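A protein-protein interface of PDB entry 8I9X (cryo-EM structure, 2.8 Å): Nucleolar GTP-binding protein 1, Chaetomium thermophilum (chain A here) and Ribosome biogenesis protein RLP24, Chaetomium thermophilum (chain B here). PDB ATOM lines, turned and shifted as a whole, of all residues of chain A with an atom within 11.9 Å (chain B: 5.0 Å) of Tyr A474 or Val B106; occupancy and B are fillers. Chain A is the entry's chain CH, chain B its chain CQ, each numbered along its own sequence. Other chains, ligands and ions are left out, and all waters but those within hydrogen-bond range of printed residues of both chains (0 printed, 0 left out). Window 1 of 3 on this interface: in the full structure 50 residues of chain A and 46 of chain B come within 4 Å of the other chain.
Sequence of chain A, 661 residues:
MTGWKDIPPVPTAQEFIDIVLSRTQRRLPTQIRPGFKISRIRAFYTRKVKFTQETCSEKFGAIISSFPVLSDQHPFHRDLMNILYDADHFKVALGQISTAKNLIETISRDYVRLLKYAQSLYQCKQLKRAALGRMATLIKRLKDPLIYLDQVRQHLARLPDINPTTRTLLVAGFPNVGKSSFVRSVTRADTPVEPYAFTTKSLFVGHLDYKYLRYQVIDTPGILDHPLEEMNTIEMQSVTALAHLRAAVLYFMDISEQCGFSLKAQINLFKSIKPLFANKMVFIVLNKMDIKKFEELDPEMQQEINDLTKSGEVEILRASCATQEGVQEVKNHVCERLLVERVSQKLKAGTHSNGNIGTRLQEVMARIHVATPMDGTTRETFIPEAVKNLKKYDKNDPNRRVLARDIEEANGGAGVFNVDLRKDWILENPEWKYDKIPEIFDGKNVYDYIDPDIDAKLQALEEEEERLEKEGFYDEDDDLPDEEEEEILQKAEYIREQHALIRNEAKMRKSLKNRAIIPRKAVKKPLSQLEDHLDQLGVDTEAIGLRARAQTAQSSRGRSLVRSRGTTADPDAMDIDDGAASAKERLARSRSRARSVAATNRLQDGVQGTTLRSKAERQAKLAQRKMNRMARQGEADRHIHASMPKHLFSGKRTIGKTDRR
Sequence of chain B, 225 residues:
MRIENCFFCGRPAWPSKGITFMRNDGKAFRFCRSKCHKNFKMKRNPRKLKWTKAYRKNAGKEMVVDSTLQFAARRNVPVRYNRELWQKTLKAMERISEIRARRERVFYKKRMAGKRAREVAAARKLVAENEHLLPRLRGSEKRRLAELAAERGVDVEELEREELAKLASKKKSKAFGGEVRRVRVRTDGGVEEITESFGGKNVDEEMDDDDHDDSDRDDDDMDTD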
ATOM      1  N   ALA A 460     -11.178  19.729 -21.405  1.00  0.00           N
ATOM      2  CA  ALA A 460     -11.315  19.277 -20.026  1.00  0.00           C
ATOM      3  C   ALA A 460     -10.163  18.357 -19.652  1.00  0.00           C
ATOM      4  O   ALA A 460      -9.669  18.385 -18.519  1.00  0.00           O
ATOM      5  CB  ALA A 460     -12.660  18.575 -19.832  1.00  0.00           C
ATOM      6  N   LEU A 461      -9.716  17.533 -20.603  1.00  0.00           N
ATOM      7  CA  LEU A 461      -8.590  16.642 -20.336  1.00  0.00           C
ATOM      8  C   LEU A 461      -7.305  17.421 -20.065  1.00  0.00           C
ATOM      9  O   LEU A 461      -6.601  17.133 -19.090  1.00  0.00           O
ATOM     10  CB  LEU A 461      -8.405  15.670 -21.500  1.00  0.00           C
ATOM     11  CG  LEU A 461      -7.228  14.700 -21.437  1.00  0.00           C
ATOM     12  CD1 LEU A 461      -7.551  13.545 -20.508  1.00  0.00           C
ATOM     13  CD2 LEU A 461      -6.901  14.192 -22.831  1.00  0.00           C
ATOM     14  N   GLU A 462      -6.970  18.410 -20.905  1.00  0.00           N
ATOM     15  CA  GLU A 462      -5.770  19.187 -20.573  1.00  0.00           C
ATOM     16  C   GLU A 462      -5.945  19.992 -19.291  1.00  0.00           C
ATOM     17  O   GLU A 462      -4.976  20.170 -18.549  1.00  0.00           O
ATOM     18  CB  GLU A 462      -5.259  20.139 -21.673  1.00  0.00           C
ATOM     19  CG  GLU A 462      -4.683  19.526 -22.956  1.00  0.00           C
ATOM     20  CD  GLU A 462      -5.696  19.167 -23.989  1.00  0.00           C
ATOM     21  OE1 GLU A 462      -6.869  19.460 -23.761  1.00  0.00           O
ATOM     22  OE2 GLU A 462      -5.316  18.599 -25.033  1.00  0.00           O
ATOM     23  N   GLU A 463      -7.145  20.506 -19.017  1.00  0.00           N
ATOM     24  CA  GLU A 463      -7.344  21.255 -17.780  1.00  0.00           C
ATOM     25  C   GLU A 463      -7.123  20.372 -16.557  1.00  0.00           C
ATOM     26  O   GLU A 463      -6.429  20.770 -15.611  1.00  0.00           O
ATOM     27  CB  GLU A 463      -8.746  21.868 -17.770  1.00  0.00           C
ATOM     28  CG  GLU A 463      -9.010  22.867 -16.650  1.00  0.00           C
ATOM     29  CD  GLU A 463      -9.413  22.212 -15.343  1.00  0.00           C
ATOM     30  OE1 GLU A 463     -10.007  21.115 -15.381  1.00  0.00           O
ATOM     31  OE2 GLU A 463      -9.139  22.803 -14.277  1.00  0.00           O
ATOM     32  N   GLU A 464      -7.683  19.158 -16.565  1.00  0.00           N
ATOM     33  CA  GLU A 464      -7.488  18.268 -15.428  1.00  0.00           C
ATOM     34  C   GLU A 464      -6.040  17.814 -15.334  1.00  0.00           C
ATOM     35  O   GLU A 464      -5.511  17.655 -14.228  1.00  0.00           O
ATOM     36  CB  GLU A 464      -8.441  17.070 -15.508  1.00  0.00           C
ATOM     37  CG  GLU A 464      -8.283  16.170 -16.716  1.00  0.00           C
ATOM     38  CD  GLU A 464      -7.225  15.106 -16.513  1.00  0.00           C
ATOM     39  OE1 GLU A 464      -6.882  14.823 -15.345  1.00  0.00           O
ATOM     40  OE2 GLU A 464      -6.738  14.548 -17.518  1.00  0.00           O
ATOM     41  N   GLU A 465      -5.372  17.629 -16.476  1.00  0.00           N
ATOM     42  CA  GLU A 465      -3.945  17.343 -16.439  1.00  0.00           C
ATOM     43  C   GLU A 465      -3.191  18.467 -15.745  1.00  0.00           C
ATOM     44  O   GLU A 465      -2.546  18.245 -14.713  1.00  0.00           O
ATOM     45  CB  GLU A 465      -3.415  17.139 -17.860  1.00  0.00           C
ATOM     46  CG  GLU A 465      -3.484  15.705 -18.352  1.00  0.00           C
ATOM     47  CD  GLU A 465      -2.622  14.765 -17.536  1.00  0.00           C
ATOM     48  OE1 GLU A 465      -1.400  14.708 -17.785  1.00  0.00           O
ATOM     49  OE2 GLU A 465      -3.168  14.083 -16.645  1.00  0.00           O
ATOM     50  N   GLU A 466      -3.356  19.698 -16.240  1.00  0.00           N
ATOM     51  CA  GLU A 466      -2.660  20.845 -15.670  1.00  0.00           C
ATOM     52  C   GLU A 466      -2.911  20.953 -14.176  1.00  0.00           C
ATOM     53  O   GLU A 466      -1.996  21.280 -13.409  1.00  0.00           O
ATOM     54  CB  GLU A 466      -3.085  22.129 -16.381  1.00  0.00           C
ATOM     55  CG  GLU A 466      -2.664  22.197 -17.837  1.00  0.00           C
ATOM     56  CD  GLU A 466      -1.161  22.277 -18.003  1.00  0.00           C
ATOM     57  OE1 GLU A 466      -0.493  22.859 -17.123  1.00  0.00           O
ATOM     58  OE2 GLU A 466      -0.646  21.752 -19.014  1.00  0.00           O
ATOM     59  N   ARG A 467      -4.134  20.651 -13.731  1.00  0.00           N
ATOM     60  CA  ARG A 467      -4.329  20.536 -12.291  1.00  0.00           C
ATOM     61  C   ARG A 467      -3.391  19.484 -11.715  1.00  0.00           C
ATOM     62  O   ARG A 467      -2.552  19.794 -10.863  1.00  0.00           O
ATOM     63  CB  ARG A 467      -5.782  20.214 -11.934  1.00  0.00           C
ATOM     64  CG  ARG A 467      -6.757  21.334 -12.229  1.00  0.00           C
ATOM     65  CD  ARG A 467      -8.169  20.998 -11.768  1.00  0.00           C
ATOM     66  NE  ARG A 467      -8.824  19.937 -12.520  1.00  0.00           N
ATOM     67  CZ  ARG A 467      -9.130  18.753 -12.009  1.00  0.00           C
ATOM     68  NH1 ARG A 467      -8.816  18.437 -10.762  1.00  0.00           N
ATOM     69  NH2 ARG A 467      -9.778  17.867 -12.760  1.00  0.00           N
ATOM     70  N   LEU A 468      -3.421  18.269 -12.270  1.00  0.00           N
ATOM     71  CA  LEU A 468      -2.627  17.178 -11.707  1.00  0.00           C
ATOM     72  C   LEU A 468      -1.167  17.584 -11.518  1.00  0.00           C
ATOM     73  O   LEU A 468      -0.569  17.294 -10.473  1.00  0.00           O
ATOM     74  CB  LEU A 468      -2.736  15.934 -12.587  1.00  0.00           C
ATOM     75  CG  LEU A 468      -4.116  15.279 -12.689  1.00  0.00           C
ATOM     76  CD1 LEU A 468      -3.997  13.805 -13.042  1.00  0.00           C
ATOM     77  CD2 LEU A 468      -4.896  15.453 -11.394  1.00  0.00           C
ATOM     78  N   GLU A 469      -0.581  18.288 -12.492  1.00  0.00           N
ATOM     79  CA  GLU A 469       0.762  18.822 -12.248  1.00  0.00           C
ATOM     80  C   GLU A 469       0.763  19.896 -11.161  1.00  0.00           C
ATOM     81  O   GLU A 469       1.720  19.989 -10.384  1.00  0.00           O
ATOM     82  CB  GLU A 469       1.471  19.359 -13.505  1.00  0.00           C
ATOM     83  CG  GLU A 469       1.888  18.346 -14.585  1.00  0.00           C
ATOM     84  CD  GLU A 469       0.810  17.976 -15.555  1.00  0.00           C
ATOM     85  OE1 GLU A 469      -0.272  18.556 -15.458  1.00  0.00           O
ATOM     86  OE2 GLU A 469       1.051  17.106 -16.417  1.00  0.00           O
ATOM     87  N   LYS A 470      -0.284  20.726 -11.080  1.00  0.00           N
ATOM     88  CA  LYS A 470      -0.210  21.838 -10.133  1.00  0.00           C
ATOM     89  C   LYS A 470      -0.247  21.337  -8.689  1.00  0.00           C
ATOM     90  O   LYS A 470       0.433  21.890  -7.818  1.00  0.00           O
ATOM     91  CB  LYS A 470      -1.312  22.878 -10.384  1.00  0.00           C
ATOM     92  CG  LYS A 470      -2.701  22.554  -9.866  1.00  0.00           C
ATOM     93  CD  LYS A 470      -3.690  23.655 -10.214  1.00  0.00           C
ATOM     94  CE  LYS A 470      -3.342  24.949  -9.494  1.00  0.00           C
ATOM     95  NZ  LYS A 470      -3.447  24.808  -8.015  1.00  0.00           N
ATOM     96  N   GLU A 471      -1.030  20.289  -8.408  1.00  0.00           N
ATOM     97  CA  GLU A 471      -0.919  19.687  -7.077  1.00  0.00           C
ATOM     98  C   GLU A 471       0.375  18.888  -6.947  1.00  0.00           C
ATOM     99  O   GLU A 471       1.079  18.988  -5.937  1.00  0.00           O
ATOM    100  CB  GLU A 471      -2.114  18.805  -6.669  1.00  0.00           C
ATOM    101  CG  GLU A 471      -3.510  19.409  -6.739  1.00  0.00           C
ATOM    102  CD  GLU A 471      -4.225  19.076  -8.014  1.00  0.00           C
ATOM    103  OE1 GLU A 471      -3.549  18.662  -8.961  1.00  0.00           O
ATOM    104  OE2 GLU A 471      -5.464  19.224  -8.067  1.00  0.00           O
ATOM    105  N   GLY A 472       0.709  18.087  -7.958  1.00  0.00           N
ATOM    106  CA  GLY A 472       1.924  17.303  -7.852  1.00  0.00           C
ATOM    107  C   GLY A 472       1.749  15.814  -8.064  1.00  0.00           C
ATOM    108  O   GLY A 472       2.565  15.021  -7.584  1.00  0.00           O
ATOM    109  N   PHE A 473       0.681  15.422  -8.763  1.00  0.00           N
ATOM    110  CA  PHE A 473       0.419  14.005  -9.004  1.00  0.00           C
ATOM    111  C   PHE A 473       1.601  13.312  -9.670  1.00  0.00           C
ATOM    112  O   PHE A 473       1.806  12.109  -9.468  1.00  0.00           O
ATOM    113  CB  PHE A 473      -0.835  13.848  -9.865  1.00  0.00           C
ATOM    114  CG  PHE A 473      -1.413  12.463  -9.851  1.00  0.00           C
ATOM    115  CD1 PHE A 473      -1.500  11.744  -8.672  1.00  0.00           C
ATOM    116  CD2 PHE A 473      -1.872  11.879 -11.020  1.00  0.00           C
ATOM    117  CE1 PHE A 473      -2.034  10.469  -8.659  1.00  0.00           C
ATOM    118  CE2 PHE A 473      -2.407  10.607 -11.014  1.00  0.00           C
ATOM    119  CZ  PHE A 473      -2.487   9.900  -9.832  1.00  0.00           C
ATOM    120  N   TYR A 474       2.384  14.042 -10.462  1.00  0.00           N
ATOM    121  CA  TYR A 474       3.511  13.474 -11.189  1.00  0.00           C
ATOM    122  C   TYR A 474       4.848  13.809 -10.538  1.00  0.00           C
ATOM    123  O   TYR A 474       5.903  13.570 -11.135  1.00  0.00           O
ATOM    124  CB  TYR A 474       3.496  13.957 -12.638  1.00  0.00           C
ATOM    125  CG  TYR A 474       2.187  13.702 -13.344  1.00  0.00           C
ATOM    126  CD1 TYR A 474       1.889  12.456 -13.876  1.00  0.00           C
ATOM    127  CD2 TYR A 474       1.245  14.712 -13.474  1.00  0.00           C
ATOM    128  CE1 TYR A 474       0.690  12.225 -14.520  1.00  0.00           C
ATOM    129  CE2 TYR A 474       0.046  14.491 -14.115  1.00  0.00           C
ATOM    130  CZ  TYR A 474      -0.227  13.248 -14.637  1.00  0.00           C
ATOM    131  OH  TYR A 474      -1.423  13.029 -15.276  1.00  0.00           O
ATOM    132  N   ASP A 475       4.827  14.358  -9.326  1.00  0.00           N
ATOM    133  CA  ASP A 475       6.048  14.779  -8.643  1.00  0.00           C
ATOM    134  C   ASP A 475       6.746  13.547  -8.082  1.00  0.00           C
ATOM    135  O   ASP A 475       6.322  12.980  -7.073  1.00  0.00           O
ATOM    136  CB  ASP A 475       5.727  15.782  -7.542  1.00  0.00           C
ATOM    137  CG  ASP A 475       6.952  16.189  -6.746  1.00  0.00           C
ATOM    138  OD1 ASP A 475       7.964  16.575  -7.367  1.00  0.00           O
ATOM    139  OD2 ASP A 475       6.903  16.122  -5.500  1.00  0.00           O
ATOM    140  N   GLU A 476       7.823  13.128  -8.743  1.00  0.00           N
ATOM    141  CA  GLU A 476       8.583  11.973  -8.286  1.00  0.00           C
ATOM    142  C   GLU A 476       9.343  12.316  -7.011  1.00  0.00           C
ATOM    143  O   GLU A 476       9.956  13.383  -6.907  1.00  0.00           O
ATOM    144  CB  GLU A 476       9.547  11.510  -9.377  1.00  0.00           C
ATOM    145  CG  GLU A 476      10.168  10.142  -9.132  1.00  0.00           C
ATOM    146  CD  GLU A 476      11.445  10.214  -8.317  1.00  0.00           C
ATOM    147  OE1 GLU A 476      12.135  11.252  -8.382  1.00  0.00           O
ATOM    148  OE2 GLU A 476      11.758   9.232  -7.610  1.00  0.00           O
ATOM    149  N   ASP A 477       9.303  11.409  -6.040  1.00  0.00           N
ATOM    150  CA  ASP A 477       9.983  11.619  -4.767  1.00  0.00           C
ATOM    151  C   ASP A 477      11.099  10.600  -4.568  1.00  0.00           C
ATOM    152  O   ASP A 477      10.872   9.392  -4.649  1.00  0.00           O
ATOM    153  CB  ASP A 477       8.987  11.543  -3.609  1.00  0.00           C
ATOM    154  CG  ASP A 477       7.739  12.368  -3.859  1.00  0.00           C
ATOM    155  OD1 ASP A 477       7.826  13.612  -3.797  1.00  0.00           O
ATOM    156  OD2 ASP A 477       6.673  11.771  -4.117  1.00  0.00           O
ATOM    157  N   ARG B 102       1.456   7.988 -19.080  1.00  0.00           N
ATOM    158  CA  ARG B 102       1.952   8.651 -17.875  1.00  0.00           C
ATOM    159  C   ARG B 102       1.110   8.293 -16.648  1.00  0.00           C
ATOM    160  O   ARG B 102       1.652   8.023 -15.565  1.00  0.00           O
ATOM    161  CB  ARG B 102       2.010  10.158 -18.120  1.00  0.00           C
ATOM    162  CG  ARG B 102       3.355  10.570 -18.718  1.00  0.00           C
ATOM    163  CD  ARG B 102       3.470  12.040 -19.117  1.00  0.00           C
ATOM    164  NE  ARG B 102       2.658  12.966 -18.339  1.00  0.00           N
ATOM    165  CZ  ARG B 102       2.897  13.301 -17.078  1.00  0.00           C
ATOM    166  NH1 ARG B 102       3.903  12.774 -16.400  1.00  0.00           N
ATOM    167  NH2 ARG B 102       2.119  14.204 -16.492  1.00  0.00           N
ATOM    168  N   ARG B 103      -0.218   8.256 -16.804  1.00  0.00           N
ATOM    169  CA  ARG B 103      -1.079   7.853 -15.692  1.00  0.00           C
ATOM    170  C   ARG B 103      -0.813   6.423 -15.248  1.00  0.00           C
ATOM    171  O   ARG B 103      -0.806   6.147 -14.045  1.00  0.00           O
ATOM    172  CB  ARG B 103      -2.557   8.004 -16.056  1.00  0.00           C
ATOM    173  CG  ARG B 103      -2.949   9.339 -16.638  1.00  0.00           C
ATOM    174  CD  ARG B 103      -3.138  10.380 -15.556  1.00  0.00           C
ATOM    175  NE  ARG B 103      -4.067  11.423 -15.970  1.00  0.00           N
ATOM    176  CZ  ARG B 103      -5.377  11.257 -16.094  1.00  0.00           C
ATOM    177  NH1 ARG B 103      -5.957  10.098 -15.822  1.00  0.00           N
ATOM    178  NH2 ARG B 103      -6.125  12.278 -16.498  1.00  0.00           N
ATOM    179  N   GLU B 104      -0.627   5.498 -16.189  1.00  0.00           N
ATOM    180  CA  GLU B 104      -0.349   4.116 -15.820  1.00  0.00           C
ATOM    181  C   GLU B 104       0.998   3.981 -15.127  1.00  0.00           C
ATOM    182  O   GLU B 104       1.131   3.186 -14.188  1.00  0.00           O
ATOM    183  CB  GLU B 104      -0.407   3.215 -17.054  1.00  0.00           C
ATOM    184  CG  GLU B 104      -0.788   1.774 -16.752  1.00  0.00           C
ATOM    185  CD  GLU B 104       0.404   0.916 -16.375  1.00  0.00           C
ATOM    186  OE1 GLU B 104       1.551   1.367 -16.570  1.00  0.00           O
ATOM    187  OE2 GLU B 104       0.192  -0.213 -15.882  1.00  0.00           O
ATOM    188  N   ARG B 105       2.005   4.732 -15.581  1.00  0.00           N
ATOM    189  CA  ARG B 105       3.268   4.793 -14.857  1.00  0.00           C
ATOM    190  C   ARG B 105       3.068   5.223 -13.411  1.00  0.00           C
ATOM    191  O   ARG B 105       3.592   4.569 -12.499  1.00  0.00           O
ATOM    192  CB  ARG B 105       4.219   5.760 -15.564  1.00  0.00           C
ATOM    193  CG  ARG B 105       5.592   5.896 -14.931  1.00  0.00           C
ATOM    194  CD  ARG B 105       6.381   4.607 -15.038  1.00  0.00           C
ATOM    195  NE  ARG B 105       7.719   4.744 -14.476  1.00  0.00           N
ATOM    196  CZ  ARG B 105       8.560   3.737 -14.291  1.00  0.00           C
ATOM    197  NH1 ARG B 105       8.234   2.497 -14.616  1.00  0.00           N
ATOM    198  NH2 ARG B 105       9.757   3.980 -13.768  1.00  0.00           N
ATOM    199  N   VAL B 106       2.299   6.291 -13.187  1.00  0.00           N
ATOM    200  CA  VAL B 106       2.030   6.738 -11.821  1.00  0.00           C
ATOM    201  C   VAL B 106       1.280   5.674 -11.023  1.00  0.00           C
ATOM    202  O   VAL B 106       1.587   5.444  -9.847  1.00  0.00           O
ATOM    203  CB  VAL B 106       1.258   8.066 -11.839  1.00  0.00           C
ATOM    204  CG1 VAL B 106       0.711   8.382 -10.460  1.00  0.00           C
ATOM    205  CG2 VAL B 106       2.155   9.189 -12.323  1.00  0.00           C
ATOM    206  N   PHE B 107       0.286   5.028 -11.633  1.00  0.00           N
ATOM    207  CA  PHE B 107      -0.481   3.997 -10.940  1.00  0.00           C
ATOM    208  C   PHE B 107       0.408   2.847 -10.494  1.00  0.00           C
ATOM    209  O   PHE B 107       0.297   2.370  -9.357  1.00  0.00           O
ATOM    210  CB  PHE B 107      -1.591   3.478 -11.851  1.00  0.00           C
ATOM    211  CG  PHE B 107      -2.624   2.651 -11.144  1.00  0.00           C
ATOM    212  CD1 PHE B 107      -3.593   3.246 -10.359  1.00  0.00           C
ATOM    213  CD2 PHE B 107      -2.622   1.275 -11.263  1.00  0.00           C
ATOM    214  CE1 PHE B 107      -4.543   2.483  -9.713  1.00  0.00           C
ATOM    215  CE2 PHE B 107      -3.567   0.507 -10.619  1.00  0.00           C
ATOM    216  CZ  PHE B 107      -4.528   1.113  -9.842  1.00  0.00           C
ATOM    217  N   TYR B 108       1.289   2.380 -11.376  1.00  0.00           N
ATOM    218  CA  TYR B 108       2.115   1.236 -11.022  1.00  0.00           C
ATOM    219  C   TYR B 108       3.167   1.632  -9.994  1.00  0.00           C
ATOM    220  O   TYR B 108       3.495   0.833  -9.108  1.00  0.00           O
ATOM    221  CB  TYR B 108       2.743   0.643 -12.284  1.00  0.00           C
ATOM    222  CG  TYR B 108       3.656  -0.536 -12.050  1.00  0.00           C
ATOM    223  CD1 TYR B 108       3.155  -1.827 -12.121  1.00  0.00           C
ATOM    224  CD2 TYR B 108       5.008  -0.374 -11.800  1.00  0.00           C
ATOM    225  CE1 TYR B 108       3.963  -2.922 -11.925  1.00  0.00           C
ATOM    226  CE2 TYR B 108       5.823  -1.468 -11.608  1.00  0.00           C
ATOM    227  CZ  TYR B 108       5.298  -2.735 -11.667  1.00  0.00           C
ATOM    228  OH  TYR B 108       6.118  -3.823 -11.470  1.00  0.00           O
ATOM    229  N   LYS B 109       3.675   2.867 -10.071  1.00  0.00           N
ATOM    230  CA  LYS B 109       4.484   3.422  -8.993  1.00  0.00           C
ATOM    231  C   LYS B 109       3.767   3.410  -7.649  1.00  0.00           C
ATOM    232  O   LYS B 109       4.353   2.966  -6.657  1.00  0.00           O
ATOM    233  CB  LYS B 109       4.886   4.862  -9.326  1.00  0.00           C
ATOM    234  CG  LYS B 109       5.774   5.526  -8.283  1.00  0.00           C
ATOM    235  CD  LYS B 109       7.100   4.813  -8.131  1.00  0.00           C
ATOM    236  CE  LYS B 109       7.915   4.933  -9.403  1.00  0.00           C
ATOM    237  NZ  LYS B 109       8.352   6.338  -9.633  1.00  0.00           N
ATOM    238  N   LYS B 110       2.523   3.878  -7.595  1.00  0.00           N
ATOM    239  CA  LYS B 110       1.748   3.852  -6.362  1.00  0.00           C
ATOM    240  C   LYS B 110       1.492   2.442  -5.854  1.00  0.00           C
ATOM    241  O   LYS B 110       1.470   2.234  -4.636  1.00  0.00           O
ATOM    242  CB  LYS B 110       0.407   4.571  -6.558  1.00  0.00           C
ATOM    243  CG  LYS B 110      -0.406   4.714  -5.286  1.00  0.00           C
ATOM    244  CD  LYS B 110      -1.714   5.439  -5.543  1.00  0.00           C
ATOM    245  CE  LYS B 110      -1.473   6.912  -5.829  1.00  0.00           C
ATOM    246  NZ  LYS B 110      -0.955   7.633  -4.631  1.00  0.00           N
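The side-chain carboxylate (OE2) of Glu A469 lies within salt-bridge range of the guanidinium group (NH2) of Arg B102, at 3.1 Å.
The guanidinium group (NH2) of Arg B103 lies within salt-bridge range of the side-chain carboxylate (OE2) of Glu A464 (2.6 Å).
OE2 of Glu A465 lies within salt-bridge range of NE of Arg B103, 2.9 Å away.
NH2 of Arg B102 lies within salt-bridge range of OE1 of Glu A465 (3.8 Å).
The side-chain hydroxyl (OH) of Tyr A474 lies close to the guanidinium group (NE) of Arg B103 (3.2 Å).
N of Leu A468 sits close to OE1 of Glu A471, at 3.3 Å.
The backbone carbonyl oxygen (O) of Glu A465 lies close to the side-chain carboxylate (OE1) of Glu A469, 2.4 Å away.
N of Glu A466 sits close to OE1 of Glu A469, 3.4 Å away.
The side-chain hydroxyl (OH) of Tyr A474 is in hydrogen-bond range of the side-chain carboxylate (OE2) of Glu A465.
O of Leu A468 sits at hydrogen-bond distance from N of Phe A473 (2.8 Å).
Leu A468 touches Arg B103.
Phe A473 touches Val B106.
NH2 of Arg B102 touches CE1 of Tyr A474, at 3.1 Å.
Val B106 touches Tyr A474 (CG2 to CD1, 3.6 Å).
Tyr A474 touches three residues of chain B.
No residue of chain A comes within 4 Å of Glu B104.
No residue of chain A comes within 4 Å of Arg B105.
No residue of chain A comes within 4 Å of Lys B109.
Printed residues of chain B within 4 Å of Glu A465: Arg B102 (3.8 Å) and Arg B103 (2.9 Å).
Printed residues of chain B within 4 Å of Leu A468: Arg B103.
Printed residues of chain B within 4 Å of Glu A464: Arg B103 (2.6 Å).
Of the printed residues of chain B, Glu A469 touches Arg B102 (3.1 Å).
Printed residues of chain B within 4 Å of Phe A473: Val B106.
Ala A460 touches none of the printed residues of chain B.
Glu A466 touches none of the printed residues of chain B.
The nearest residue of chain A that does not touch Val B106 is Asp A475 (6.5 Å).
Printed residues of chain B that touch a printed residue of chain A: Arg B102, Arg B103 and Val B106.
Among the printed residues, 9 pairs touch across the chains.
Among the printed residues, Asp or Glu carboxylates within 4 Å of a Lys or Arg side-chain nitrogen of the other chain: Glu A464 with Arg B103, Glu A465 with Arg B102, Glu A465 with Arg B103 and Glu A469 with Arg B102.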
